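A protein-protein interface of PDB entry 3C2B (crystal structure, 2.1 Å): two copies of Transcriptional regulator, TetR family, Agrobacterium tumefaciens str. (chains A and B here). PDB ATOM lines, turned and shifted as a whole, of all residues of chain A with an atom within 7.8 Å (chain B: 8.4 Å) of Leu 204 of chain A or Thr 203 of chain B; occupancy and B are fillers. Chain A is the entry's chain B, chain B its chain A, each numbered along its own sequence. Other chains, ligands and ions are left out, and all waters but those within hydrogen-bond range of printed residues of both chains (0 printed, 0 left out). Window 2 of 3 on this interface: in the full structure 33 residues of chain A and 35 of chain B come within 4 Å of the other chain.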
ATOM      1  N   LEU A 156       5.455 -16.513  30.405  1.00  0.00           N
ATOM      2  CA  LEU A 156       5.542 -17.849  29.914  1.00  0.00           C
ATOM      3  C   LEU A 156       4.156 -18.232  29.441  1.00  0.00           C
ATOM      4  O   LEU A 156       3.155 -17.828  30.028  1.00  0.00           O
ATOM      5  CB  LEU A 156       6.017 -18.821  31.017  1.00  0.00           C
ATOM      6  CG  LEU A 156       7.373 -18.664  31.692  1.00  0.00           C
ATOM      7  CD1 LEU A 156       7.543 -19.749  32.757  1.00  0.00           C
ATOM      8  CD2 LEU A 156       8.485 -18.739  30.685  1.00  0.00           C
ATOM      9  N   ARG A 157       4.107 -19.017  28.385  1.00  0.00           N
ATOM     10  CA  ARG A 157       2.843 -19.515  27.875  1.00  0.00           C
ATOM     11  C   ARG A 157       2.987 -21.024  27.626  1.00  0.00           C
ATOM     12  O   ARG A 157       3.950 -21.493  27.027  1.00  0.00           O
ATOM     13  CB  ARG A 157       2.408 -18.717  26.611  1.00  0.00           C
ATOM     14  CG  ARG A 157       1.071 -19.163  25.914  1.00  0.00           C
ATOM     15  CD  ARG A 157       0.153 -17.967  25.433  1.00  0.00           C
ATOM     16  NE  ARG A 157       0.821 -16.884  24.678  1.00  0.00           N
ATOM     17  CZ  ARG A 157       0.953 -15.616  25.100  1.00  0.00           C
ATOM     18  NH1 ARG A 157       0.484 -15.220  26.291  1.00  0.00           N
ATOM     19  NH2 ARG A 157       1.574 -14.729  24.328  1.00  0.00           N
ATOM     20  N   PHE A 158       2.051 -21.786  28.150  1.00  0.00           N
ATOM     21  CA  PHE A 158       2.052 -23.217  27.915  1.00  0.00           C
ATOM     22  C   PHE A 158       0.653 -23.711  28.247  1.00  0.00           C
ATOM     23  O   PHE A 158      -0.046 -23.140  29.094  1.00  0.00           O
ATOM     24  CB  PHE A 158       3.108 -23.940  28.788  1.00  0.00           C
ATOM     25  CG  PHE A 158       3.076 -23.540  30.257  1.00  0.00           C
ATOM     26  CD1 PHE A 158       3.946 -22.573  30.759  1.00  0.00           C
ATOM     27  CD2 PHE A 158       2.157 -24.098  31.118  1.00  0.00           C
ATOM     28  CE1 PHE A 158       3.915 -22.217  32.075  1.00  0.00           C
ATOM     29  CE2 PHE A 158       2.109 -23.729  32.453  1.00  0.00           C
ATOM     30  CZ  PHE A 158       2.985 -22.795  32.935  1.00  0.00           C
ATOM     31  N   ALA A 164       5.616 -28.365  30.342  1.00  0.00           N
ATOM     32  CA  ALA A 164       6.602 -27.303  30.363  1.00  0.00           C
ATOM     33  C   ALA A 164       7.764 -27.723  31.251  1.00  0.00           C
ATOM     34  O   ALA A 164       8.902 -27.478  30.918  1.00  0.00           O
ATOM     35  CB  ALA A 164       6.006 -26.057  30.912  1.00  0.00           C
ATOM     36  N   SER A 167       9.932 -30.540  29.649  1.00  0.00           N
ATOM     37  CA  SER A 167      10.876 -29.925  28.712  1.00  0.00           C
ATOM     38  C   SER A 167      12.058 -29.265  29.400  1.00  0.00           C
ATOM     39  O   SER A 167      13.195 -29.467  28.983  1.00  0.00           O
ATOM     40  CB  SER A 167      10.190 -28.848  27.852  1.00  0.00           C
ATOM     41  OG  SER A 167       9.192 -29.433  27.046  1.00  0.00           O
ATOM     42  N   PHE A 168      11.782 -28.455  30.424  1.00  0.00           N
ATOM     43  CA  PHE A 168      12.838 -27.766  31.172  1.00  0.00           C
ATOM     44  C   PHE A 168      13.803 -28.773  31.790  1.00  0.00           C
ATOM     45  O   PHE A 168      15.042 -28.653  31.665  1.00  0.00           O
ATOM     46  CB  PHE A 168      12.207 -26.885  32.265  1.00  0.00           C
ATOM     47  CG  PHE A 168      13.167 -25.920  32.930  1.00  0.00           C
ATOM     48  CD1 PHE A 168      14.247 -25.381  32.224  1.00  0.00           C
ATOM     49  CD2 PHE A 168      12.971 -25.540  34.263  1.00  0.00           C
ATOM     50  CE1 PHE A 168      15.108 -24.429  32.834  1.00  0.00           C
ATOM     51  CE2 PHE A 168      13.825 -24.612  34.895  1.00  0.00           C
ATOM     52  CZ  PHE A 168      14.897 -24.064  34.172  1.00  0.00           C
ATOM     53  N   LEU A 171      15.985 -30.299  29.099  1.00  0.00           N
ATOM     54  CA  LEU A 171      16.978 -29.308  28.696  1.00  0.00           C
ATOM     55  C   LEU A 171      18.136 -29.149  29.665  1.00  0.00           C
ATOM     56  O   LEU A 171      19.268 -28.992  29.238  1.00  0.00           O
ATOM     57  CB  LEU A 171      16.315 -27.947  28.384  1.00  0.00           C
ATOM     58  CG  LEU A 171      15.383 -27.937  27.159  1.00  0.00           C
ATOM     59  CD1 LEU A 171      14.450 -26.701  27.238  1.00  0.00           C
ATOM     60  CD2 LEU A 171      16.141 -28.078  25.765  1.00  0.00           C
ATOM     61  N   ALA A 197      20.238 -23.844  29.450  1.00  0.00           N
ATOM     62  CA  ALA A 197      18.928 -24.480  29.557  1.00  0.00           C
ATOM     63  C   ALA A 197      17.802 -23.466  29.697  1.00  0.00           C
ATOM     64  O   ALA A 197      16.701 -23.636  29.140  1.00  0.00           O
ATOM     65  CB  ALA A 197      18.906 -25.455  30.709  1.00  0.00           C
ATOM     66  N   VAL A 198      18.073 -22.405  30.432  1.00  0.00           N
ATOM     67  CA  VAL A 198      17.084 -21.371  30.620  1.00  0.00           C
ATOM     68  C   VAL A 198      16.856 -20.569  29.310  1.00  0.00           C
ATOM     69  O   VAL A 198      15.716 -20.259  28.957  1.00  0.00           O
ATOM     70  CB  VAL A 198      17.479 -20.492  31.768  1.00  0.00           C
ATOM     71  CG1 VAL A 198      16.638 -19.239  31.794  1.00  0.00           C
ATOM     72  CG2 VAL A 198      17.344 -21.290  33.081  1.00  0.00           C
ATOM     73  N   VAL A 199      17.922 -20.283  28.564  1.00  0.00           N
ATOM     74  CA  VAL A 199      17.770 -19.670  27.226  1.00  0.00           C
ATOM     75  C   VAL A 199      16.890 -20.576  26.345  1.00  0.00           C
ATOM     76  O   VAL A 199      15.952 -20.093  25.706  1.00  0.00           O
ATOM     77  CB  VAL A 199      19.149 -19.422  26.527  1.00  0.00           C
ATOM     78  CG1 VAL A 199      18.981 -19.112  24.985  1.00  0.00           C
ATOM     79  CG2 VAL A 199      19.953 -18.301  27.247  1.00  0.00           C
ATOM     80  N   ALA A 200      17.165 -21.881  26.314  1.00  0.00           N
ATOM     81  CA  ALA A 200      16.318 -22.766  25.469  1.00  0.00           C
ATOM     82  C   ALA A 200      14.883 -22.826  25.965  1.00  0.00           C
ATOM     83  O   ALA A 200      13.971 -22.906  25.171  1.00  0.00           O
ATOM     84  CB  ALA A 200      16.884 -24.185  25.345  1.00  0.00           C
ATOM     85  N   PHE A 201      14.700 -22.856  27.275  1.00  0.00           N
ATOM     86  CA  PHE A 201      13.392 -22.914  27.863  1.00  0.00           C
ATOM     87  C   PHE A 201      12.569 -21.669  27.568  1.00  0.00           C
ATOM     88  O   PHE A 201      11.413 -21.756  27.222  1.00  0.00           O
ATOM     89  CB  PHE A 201      13.526 -23.135  29.361  1.00  0.00           C
ATOM     90  CG  PHE A 201      12.216 -23.156  30.070  1.00  0.00           C
ATOM     91  CD1 PHE A 201      11.381 -24.254  29.953  1.00  0.00           C
ATOM     92  CD2 PHE A 201      11.793 -22.053  30.809  1.00  0.00           C
ATOM     93  CE1 PHE A 201      10.189 -24.260  30.585  1.00  0.00           C
ATOM     94  CE2 PHE A 201      10.571 -22.076  31.466  1.00  0.00           C
ATOM     95  CZ  PHE A 201       9.783 -23.157  31.363  1.00  0.00           C
ATOM     96  N   LEU A 202      13.188 -20.499  27.670  1.00  0.00           N
ATOM     97  CA  LEU A 202      12.524 -19.245  27.269  1.00  0.00           C
ATOM     98  C   LEU A 202      12.291 -19.104  25.787  1.00  0.00           C
ATOM     99  O   LEU A 202      11.374 -18.407  25.403  1.00  0.00           O
ATOM    100  CB  LEU A 202      13.263 -17.997  27.817  1.00  0.00           C
ATOM    101  CG  LEU A 202      13.390 -17.975  29.349  1.00  0.00           C
ATOM    102  CD1 LEU A 202      14.205 -16.749  29.789  1.00  0.00           C
ATOM    103  CD2 LEU A 202      12.001 -17.972  30.020  1.00  0.00           C
ATOM    104  N   THR A 203      13.068 -19.775  24.938  1.00  0.00           N
ATOM    105  CA  THR A 203      12.739 -19.786  23.508  1.00  0.00           C
ATOM    106  C   THR A 203      11.439 -20.589  23.282  1.00  0.00           C
ATOM    107  O   THR A 203      10.598 -20.193  22.493  1.00  0.00           O
ATOM    108  CB  THR A 203      13.943 -20.340  22.610  1.00  0.00           C
ATOM    109  OG1 THR A 203      15.126 -19.604  22.880  1.00  0.00           O
ATOM    110  CG2 THR A 203      13.667 -20.286  21.067  1.00  0.00           C
ATOM    111  N   LEU A 204      11.276 -21.712  23.983  1.00  0.00           N
ATOM    112  CA  LEU A 204      10.123 -22.601  23.788  1.00  0.00           C
ATOM    113  C   LEU A 204       8.849 -22.061  24.435  1.00  0.00           C
ATOM    114  O   LEU A 204       7.767 -22.125  23.821  1.00  0.00           O
ATOM    115  CB  LEU A 204      10.406 -23.998  24.395  1.00  0.00           C
ATOM    116  CG  LEU A 204      11.493 -24.841  23.746  1.00  0.00           C
ATOM    117  CD1 LEU A 204      11.673 -26.230  24.464  1.00  0.00           C
ATOM    118  CD2 LEU A 204      11.190 -25.005  22.224  1.00  0.00           C
ATOM    119  N   TYR A 205       8.972 -21.529  25.656  1.00  0.00           N
ATOM    120  CA  TYR A 205       7.800 -21.116  26.482  1.00  0.00           C
ATOM    121  C   TYR A 205       7.732 -19.627  26.792  1.00  0.00           C
ATOM    122  O   TYR A 205       6.733 -19.140  27.375  1.00  0.00           O
ATOM    123  CB  TYR A 205       7.726 -21.912  27.780  1.00  0.00           C
ATOM    124  CG  TYR A 205       7.584 -23.399  27.531  1.00  0.00           C
ATOM    125  CD1 TYR A 205       6.360 -23.940  27.165  1.00  0.00           C
ATOM    126  CD2 TYR A 205       8.679 -24.233  27.573  1.00  0.00           C
ATOM    127  CE1 TYR A 205       6.219 -25.277  26.896  1.00  0.00           C
ATOM    128  CE2 TYR A 205       8.565 -25.589  27.283  1.00  0.00           C
ATOM    129  CZ  TYR A 205       7.310 -26.112  26.951  1.00  0.00           C
ATOM    130  OH  TYR A 205       7.136 -27.462  26.677  1.00  0.00           O
ATOM    131  N   GLY A 206       8.788 -18.917  26.426  1.00  0.00           N
ATOM    132  CA  GLY A 206       8.879 -17.503  26.684  1.00  0.00           C
ATOM    133  C   GLY A 206       7.979 -16.685  25.780  1.00  0.00           C
ATOM    134  O   GLY A 206       7.883 -16.877  24.550  1.00  0.00           O
ATOM    135  N   THR A 207       7.339 -15.724  26.404  1.00  0.00           N
ATOM    136  CA  THR A 207       6.368 -14.863  25.789  1.00  0.00           C
ATOM    137  C   THR A 207       7.081 -13.644  25.143  1.00  0.00           C
ATOM    138  O   THR A 207       8.208 -13.306  25.512  1.00  0.00           O
ATOM    139  CB  THR A 207       5.457 -14.471  26.946  1.00  0.00           C
ATOM    140  OG1 THR A 207       4.088 -14.682  26.624  1.00  0.00           O
ATOM    141  CG2 THR A 207       5.734 -13.137  27.469  1.00  0.00           C
ATOM    142  N   HIS A 211      10.793 -11.706  26.336  1.00  0.00           N
ATOM    143  CA  HIS A 211      11.895 -11.416  25.443  1.00  0.00           C
ATOM    144  C   HIS A 211      12.103  -9.906  25.266  1.00  0.00           C
ATOM    145  O   HIS A 211      13.258  -9.446  25.223  1.00  0.00           O
ATOM    146  CB  HIS A 211      11.740 -12.130  24.091  1.00  0.00           C
ATOM    147  CG  HIS A 211      11.710 -13.616  24.214  1.00  0.00           C
ATOM    148  ND1 HIS A 211      12.812 -14.348  24.600  1.00  0.00           N
ATOM    149  CD2 HIS A 211      10.709 -14.505  24.037  1.00  0.00           C
ATOM    150  CE1 HIS A 211      12.492 -15.629  24.648  1.00  0.00           C
ATOM    151  NE2 HIS A 211      11.223 -15.751  24.301  1.00  0.00           N
ATOM    152  N   TYR B 155      18.295 -26.264   6.808  1.00  0.00           N
ATOM    153  CA  TYR B 155      17.085 -26.326   7.674  1.00  0.00           C
ATOM    154  C   TYR B 155      17.336 -26.165   9.185  1.00  0.00           C
ATOM    155  O   TYR B 155      16.417 -25.858   9.922  1.00  0.00           O
ATOM    156  CB  TYR B 155      16.285 -27.614   7.427  1.00  0.00           C
ATOM    157  CG  TYR B 155      15.799 -27.790   6.007  1.00  0.00           C
ATOM    158  CD1 TYR B 155      14.974 -26.828   5.387  1.00  0.00           C
ATOM    159  CD2 TYR B 155      16.153 -28.936   5.277  1.00  0.00           C
ATOM    160  CE1 TYR B 155      14.534 -27.004   4.080  1.00  0.00           C
ATOM    161  CE2 TYR B 155      15.709 -29.117   3.980  1.00  0.00           C
ATOM    162  CZ  TYR B 155      14.913 -28.153   3.383  1.00  0.00           C
ATOM    163  OH  TYR B 155      14.495 -28.373   2.094  1.00  0.00           O
ATOM    164  N   LEU B 156      18.576 -26.372   9.620  1.00  0.00           N
ATOM    165  CA  LEU B 156      18.970 -26.269  11.039  1.00  0.00           C
ATOM    166  C   LEU B 156      20.158 -25.344  11.214  1.00  0.00           C
ATOM    167  O   LEU B 156      21.106 -25.381  10.431  1.00  0.00           O
ATOM    168  CB  LEU B 156      19.371 -27.636  11.611  1.00  0.00           C
ATOM    169  CG  LEU B 156      18.330 -28.737  11.595  1.00  0.00           C
ATOM    170  CD1 LEU B 156      18.993 -29.974  12.182  1.00  0.00           C
ATOM    171  CD2 LEU B 156      17.109 -28.288  12.414  1.00  0.00           C
ATOM    172  N   ARG B 157      20.104 -24.543  12.266  1.00  0.00           N
ATOM    173  CA  ARG B 157      21.188 -23.660  12.594  1.00  0.00           C
ATOM    174  C   ARG B 157      21.566 -23.910  14.051  1.00  0.00           C
ATOM    175  O   ARG B 157      20.691 -24.014  14.901  1.00  0.00           O
ATOM    176  CB  ARG B 157      20.749 -22.196  12.344  1.00  0.00           C
ATOM    177  CG  ARG B 157      21.409 -21.168  13.226  1.00  0.00           C
ATOM    178  CD  ARG B 157      20.765 -19.743  13.159  1.00  0.00           C
ATOM    179  NE  ARG B 157      19.336 -19.635  13.532  1.00  0.00           N
ATOM    180  CZ  ARG B 157      18.770 -20.045  14.680  1.00  0.00           C
ATOM    181  NH1 ARG B 157      19.468 -20.673  15.635  1.00  0.00           N
ATOM    182  NH2 ARG B 157      17.464 -19.844  14.864  1.00  0.00           N
ATOM    183  N   SER B 167      20.198 -31.229  23.491  1.00  0.00           N
ATOM    184  CA  SER B 167      18.873 -30.652  23.656  1.00  0.00           C
ATOM    185  C   SER B 167      17.789 -31.603  23.137  1.00  0.00           C
ATOM    186  O   SER B 167      16.820 -31.850  23.824  1.00  0.00           O
ATOM    187  CB  SER B 167      18.745 -29.329  22.902  1.00  0.00           C
ATOM    188  OG  SER B 167      19.555 -28.313  23.487  1.00  0.00           O
ATOM    189  N   LEU B 171      14.865 -33.345  25.344  1.00  0.00           N
ATOM    190  CA  LEU B 171      13.467 -33.113  24.922  1.00  0.00           C
ATOM    191  C   LEU B 171      12.681 -34.398  24.636  1.00  0.00           C
ATOM    192  O   LEU B 171      11.498 -34.492  24.974  1.00  0.00           O
ATOM    193  CB  LEU B 171      13.366 -32.167  23.717  1.00  0.00           C
ATOM    194  CG  LEU B 171      13.813 -30.698  23.941  1.00  0.00           C
ATOM    195  CD1 LEU B 171      13.924 -29.960  22.586  1.00  0.00           C
ATOM    196  CD2 LEU B 171      12.827 -29.898  24.867  1.00  0.00           C
ATOM    197  N   LYS B 196       6.031 -34.194  19.574  1.00  0.00           N
ATOM    198  CA  LYS B 196       6.227 -33.039  20.474  1.00  0.00           C
ATOM    199  C   LYS B 196       7.692 -32.635  20.568  1.00  0.00           C
ATOM    200  O   LYS B 196       8.027 -31.450  20.489  1.00  0.00           O
ATOM    201  CB  LYS B 196       5.687 -33.362  21.866  1.00  0.00           C
ATOM    202  CG  LYS B 196       4.166 -33.458  21.885  1.00  0.00           C
ATOM    203  CD  LYS B 196       3.593 -33.844  23.280  1.00  0.00           C
ATOM    204  CE  LYS B 196       2.070 -33.808  23.235  1.00  0.00           C
ATOM    205  NZ  LYS B 196       1.480 -34.701  24.269  1.00  0.00           N
ATOM    206  N   ALA B 197       8.578 -33.628  20.705  1.00  0.00           N
ATOM    207  CA  ALA B 197      10.019 -33.349  20.809  1.00  0.00           C
ATOM    208  C   ALA B 197      10.621 -32.738  19.479  1.00  0.00           C
ATOM    209  O   ALA B 197      11.522 -31.883  19.513  1.00  0.00           O
ATOM    210  CB  ALA B 197      10.723 -34.616  21.205  1.00  0.00           C
ATOM    211  N   VAL B 198      10.088 -33.177  18.340  1.00  0.00           N
ATOM    212  CA  VAL B 198      10.468 -32.663  17.032  1.00  0.00           C
ATOM    213  C   VAL B 198       9.994 -31.234  16.836  1.00  0.00           C
ATOM    214  O   VAL B 198      10.797 -30.416  16.358  1.00  0.00           O
ATOM    215  CB  VAL B 198      10.069 -33.613  15.866  1.00  0.00           C
ATOM    216  CG1 VAL B 198      10.381 -32.987  14.483  1.00  0.00           C
ATOM    217  CG2 VAL B 198      10.867 -34.894  15.986  1.00  0.00           C
ATOM    218  N   VAL B 199       8.742 -30.923  17.223  1.00  0.00           N
ATOM    219  CA  VAL B 199       8.233 -29.526  17.213  1.00  0.00           C
ATOM    220  C   VAL B 199       9.139 -28.592  18.054  1.00  0.00           C
ATOM    221  O   VAL B 199       9.565 -27.529  17.581  1.00  0.00           O
ATOM    222  CB  VAL B 199       6.730 -29.412  17.671  1.00  0.00           C
ATOM    223  CG1 VAL B 199       6.258 -27.972  17.758  1.00  0.00           C
ATOM    224  CG2 VAL B 199       5.816 -30.151  16.690  1.00  0.00           C
ATOM    225  N   ALA B 200       9.454 -29.009  19.282  1.00  0.00           N
ATOM    226  CA  ALA B 200      10.353 -28.253  20.163  1.00  0.00           C
ATOM    227  C   ALA B 200      11.799 -28.087  19.553  1.00  0.00           C
ATOM    228  O   ALA B 200      12.343 -26.987  19.501  1.00  0.00           O
ATOM    229  CB  ALA B 200      10.394 -28.908  21.573  1.00  0.00           C
ATOM    230  N   PHE B 201      12.400 -29.181  19.126  1.00  0.00           N
ATOM    231  CA  PHE B 201      13.718 -29.152  18.467  1.00  0.00           C
ATOM    232  C   PHE B 201      13.785 -28.184  17.270  1.00  0.00           C
ATOM    233  O   PHE B 201      14.762 -27.447  17.101  1.00  0.00           O
ATOM    234  CB  PHE B 201      14.110 -30.570  18.036  1.00  0.00           C
ATOM    235  CG  PHE B 201      15.500 -30.665  17.437  1.00  0.00           C
ATOM    236  CD1 PHE B 201      16.628 -30.456  18.217  1.00  0.00           C
ATOM    237  CD2 PHE B 201      15.676 -30.910  16.081  1.00  0.00           C
ATOM    238  CE1 PHE B 201      17.922 -30.540  17.644  1.00  0.00           C
ATOM    239  CE2 PHE B 201      16.960 -30.971  15.518  1.00  0.00           C
ATOM    240  CZ  PHE B 201      18.074 -30.784  16.303  1.00  0.00           C
ATOM    241  N   LEU B 202      12.722 -28.136  16.479  1.00  0.00           N
ATOM    242  CA  LEU B 202      12.661 -27.289  15.285  1.00  0.00           C
ATOM    243  C   LEU B 202      12.432 -25.816  15.627  1.00  0.00           C
ATOM    244  O   LEU B 202      12.912 -24.921  14.931  1.00  0.00           O
ATOM    245  CB  LEU B 202      11.610 -27.834  14.300  1.00  0.00           C
ATOM    246  CG  LEU B 202      11.997 -29.164  13.611  1.00  0.00           C
ATOM    247  CD1 LEU B 202      10.951 -29.604  12.566  1.00  0.00           C
ATOM    248  CD2 LEU B 202      13.390 -29.107  12.926  1.00  0.00           C
ATOM    249  N   THR B 203      11.695 -25.561  16.707  1.00  0.00           N
ATOM    250  CA  THR B 203      11.604 -24.230  17.276  1.00  0.00           C
ATOM    251  C   THR B 203      12.985 -23.722  17.694  1.00  0.00           C
ATOM    252  O   THR B 203      13.343 -22.590  17.411  1.00  0.00           O
ATOM    253  CB  THR B 203      10.630 -24.205  18.454  1.00  0.00           C
ATOM    254  OG1 THR B 203       9.351 -24.640  17.986  1.00  0.00           O
ATOM    255  CG2 THR B 203      10.503 -22.793  19.023  1.00  0.00           C
ATOM    256  N   LEU B 204      13.770 -24.573  18.329  1.00  0.00           N
ATOM    257  CA  LEU B 204      15.076 -24.163  18.856  1.00  0.00           C
ATOM    258  C   LEU B 204      16.099 -23.943  17.752  1.00  0.00           C
ATOM    259  O   LEU B 204      16.786 -22.953  17.729  1.00  0.00           O
ATOM    260  CB  LEU B 204      15.574 -25.242  19.816  1.00  0.00           C
ATOM    261  CG  LEU B 204      15.608 -25.088  21.336  1.00  0.00           C
ATOM    262  CD1 LEU B 204      14.737 -23.989  21.897  1.00  0.00           C
ATOM    263  CD2 LEU B 204      15.392 -26.385  22.059  1.00  0.00           C
ATOM    264  N   TYR B 205      16.195 -24.885  16.828  1.00  0.00           N
ATOM    265  CA  TYR B 205      17.266 -24.911  15.842  1.00  0.00           C
ATOM    266  C   TYR B 205      16.775 -24.834  14.400  1.00  0.00           C
ATOM    267  O   TYR B 205      17.581 -24.935  13.495  1.00  0.00           O
ATOM    268  CB  TYR B 205      18.109 -26.185  15.992  1.00  0.00           C
ATOM    269  CG  TYR B 205      18.680 -26.329  17.370  1.00  0.00           C
ATOM    270  CD1 TYR B 205      19.771 -25.574  17.773  1.00  0.00           C
ATOM    271  CD2 TYR B 205      18.089 -27.174  18.301  1.00  0.00           C
ATOM    272  CE1 TYR B 205      20.294 -25.682  19.092  1.00  0.00           C
ATOM    273  CE2 TYR B 205      18.578 -27.263  19.595  1.00  0.00           C
ATOM    274  CZ  TYR B 205      19.679 -26.534  19.988  1.00  0.00           C
ATOM    275  OH  TYR B 205      20.186 -26.675  21.266  1.00  0.00           O
ATOM    276  N   GLY B 206      15.476 -24.662  14.186  1.00  0.00           N
ATOM    277  CA  GLY B 206      14.982 -24.585  12.829  1.00  0.00           C
ATOM    278  C   GLY B 206      15.226 -23.206  12.230  1.00  0.00           C
ATOM    279  O   GLY B 206      14.991 -22.202  12.872  1.00  0.00           O
ATOM    280  N   THR B 207      15.689 -23.176  10.984  1.00  0.00           N
ATOM    281  CA  THR B 207      15.872 -21.926  10.265  1.00  0.00           C
ATOM    282  C   THR B 207      14.538 -21.525   9.639  1.00  0.00           C
ATOM    283  O   THR B 207      13.626 -22.338   9.501  1.00  0.00           O
ATOM    284  CB  THR B 207      16.884 -22.089   9.111  1.00  0.00           C
ATOM    285  OG1 THR B 207      16.324 -22.973   8.141  1.00  0.00           O
ATOM    286  CG2 THR B 207      18.206 -22.659   9.592  1.00  0.00           C
ATOM    287  N   VAL B 210      13.224 -24.041   6.984  1.00  0.00           N
ATOM    288  CA  VAL B 210      12.523 -25.251   7.411  1.00  0.00           C
ATOM    289  C   VAL B 210      11.058 -24.961   7.760  1.00  0.00           C
ATOM    290  O   VAL B 210      10.186 -25.726   7.397  1.00  0.00           O
ATOM    291  CB  VAL B 210      13.260 -26.016   8.534  1.00  0.00           C
ATOM    292  CG1 VAL B 210      12.988 -25.396   9.917  1.00  0.00           C
ATOM    293  CG2 VAL B 210      12.850 -27.490   8.534  1.00  0.00           C
ATOM    294  N   HIS B 211      10.798 -23.831   8.418  1.00  0.00           N
ATOM    295  CA  HIS B 211       9.451 -23.472   8.862  1.00  0.00           C
ATOM    296  C   HIS B 211       8.545 -23.038   7.699  1.00  0.00           C
ATOM    297  O   HIS B 211       7.380 -23.460   7.611  1.00  0.00           O
ATOM    298  CB  HIS B 211       9.503 -22.402   9.957  1.00  0.00           C
ATOM    299  CG  HIS B 211      10.159 -22.871  11.234  1.00  0.00           C
ATOM    300  ND1 HIS B 211       9.777 -24.021  11.895  1.00  0.00           N
ATOM    301  CD2 HIS B 211      11.159 -22.332  11.970  1.00  0.00           C
ATOM    302  CE1 HIS B 211      10.536 -24.185  12.965  1.00  0.00           C
ATOM    303  NE2 HIS B 211      11.380 -23.172  13.035  1.00  0.00           N
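Of the 19 printed residues of chain B, 4 touch a printed residue of chain A.
Hydrophobic or aromatic side chains of chain B within 4 Å of the printed part of chain A: Leu 171 and Leu 204.
Of the 19 printed residues of chain A, 4 touch a printed residue of chain B.
Printed residues of chain A that touch a printed residue of chain B: Leu 171, Ala 200, Thr 203 and Leu 204.
Leu 204 of chain A touches just these residues of chain B: Leu 171 (3.9 Å), Ala 200 (3.6 Å), Thr 203 (3.9 Å) and Leu 204 (3.7 Å).
Of the printed residues of chain A, Thr 203 of chain B touches Leu 204.
Of the printed residues of chain B, Thr 203 of chain A touches Leu 204 (3.8 Å).
Printed residues of chain A within 4 Å of Leu 171 of chain B: Leu 171 and Leu 204.
Of the printed residues of chain B, Ala 200 of chain A touches Leu 204.
Of the printed residues of chain A, Leu 204 of chain B touches Ala 200, Thr 203 and Leu 204.
Phe 158 of chain A touches none of the printed residues of chain B.
Val 199 of chain B touches none of the printed residues of chain A.
The nearest residue of chain B that does not touch Leu 204 of chain A is Phe 201 of chain B (5.3 Å).
The nearest residue of chain A that does not touch Thr 203 of chain B is Thr 203 of chain A (4.3 Å).
The side-chain hydroxyl of Thr 203 of chain B sits at hydrogen-bond distance from the backbone carbonyl oxygen of Val 199 of chain B, 2.9 Å away.
The backbone carbonyl oxygen of Val 199 of chain A is in hydrogen-bond range of the side-chain hydroxyl of Thr 203 of chain A (3.0 Å).
Leu 171 of chain A touches its own counterpart, Leu 171 of chain B.
Ala 200 of chain A touches Leu 204 of chain B, and with the chains exchanged Leu 204 of chain A touches Ala 200 of chain B.
Thr 203 of chain A touches Leu 204 of chain B, and with the chains exchanged Leu 204 of chain A touches Thr 203 of chain B.
Leu 204 of chain A touches Leu 171 of chain B, but with the chains exchanged Leu 171 of chain A does not touch Leu 204 of chain B (4.1 Å).
Positions printed for both chains: 156, 157, 167, 171, 197, 198, 199, 200, 201, 202, 203, 204, 205, 206, 207 and 211.
Leu 171 of chain A touches Leu 171 of chain B.
Ala 200 of chain A touches Leu 204 of chain B.
CB of Thr 203 of chain A touches CD1 of Leu 204 of chain B (3.8 Å).
Leu 171 of chain B touches Leu 204 of chain A (CD2 to CD1, 3.9 Å).
Leu 204 of chain A touches Ala 200 of chain B.
CB of Thr 203 of chain B touches CD2 of Leu 204 of chain A, at 3.9 Å.
Leu 204 of chain A touches Leu 204 of chain B.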
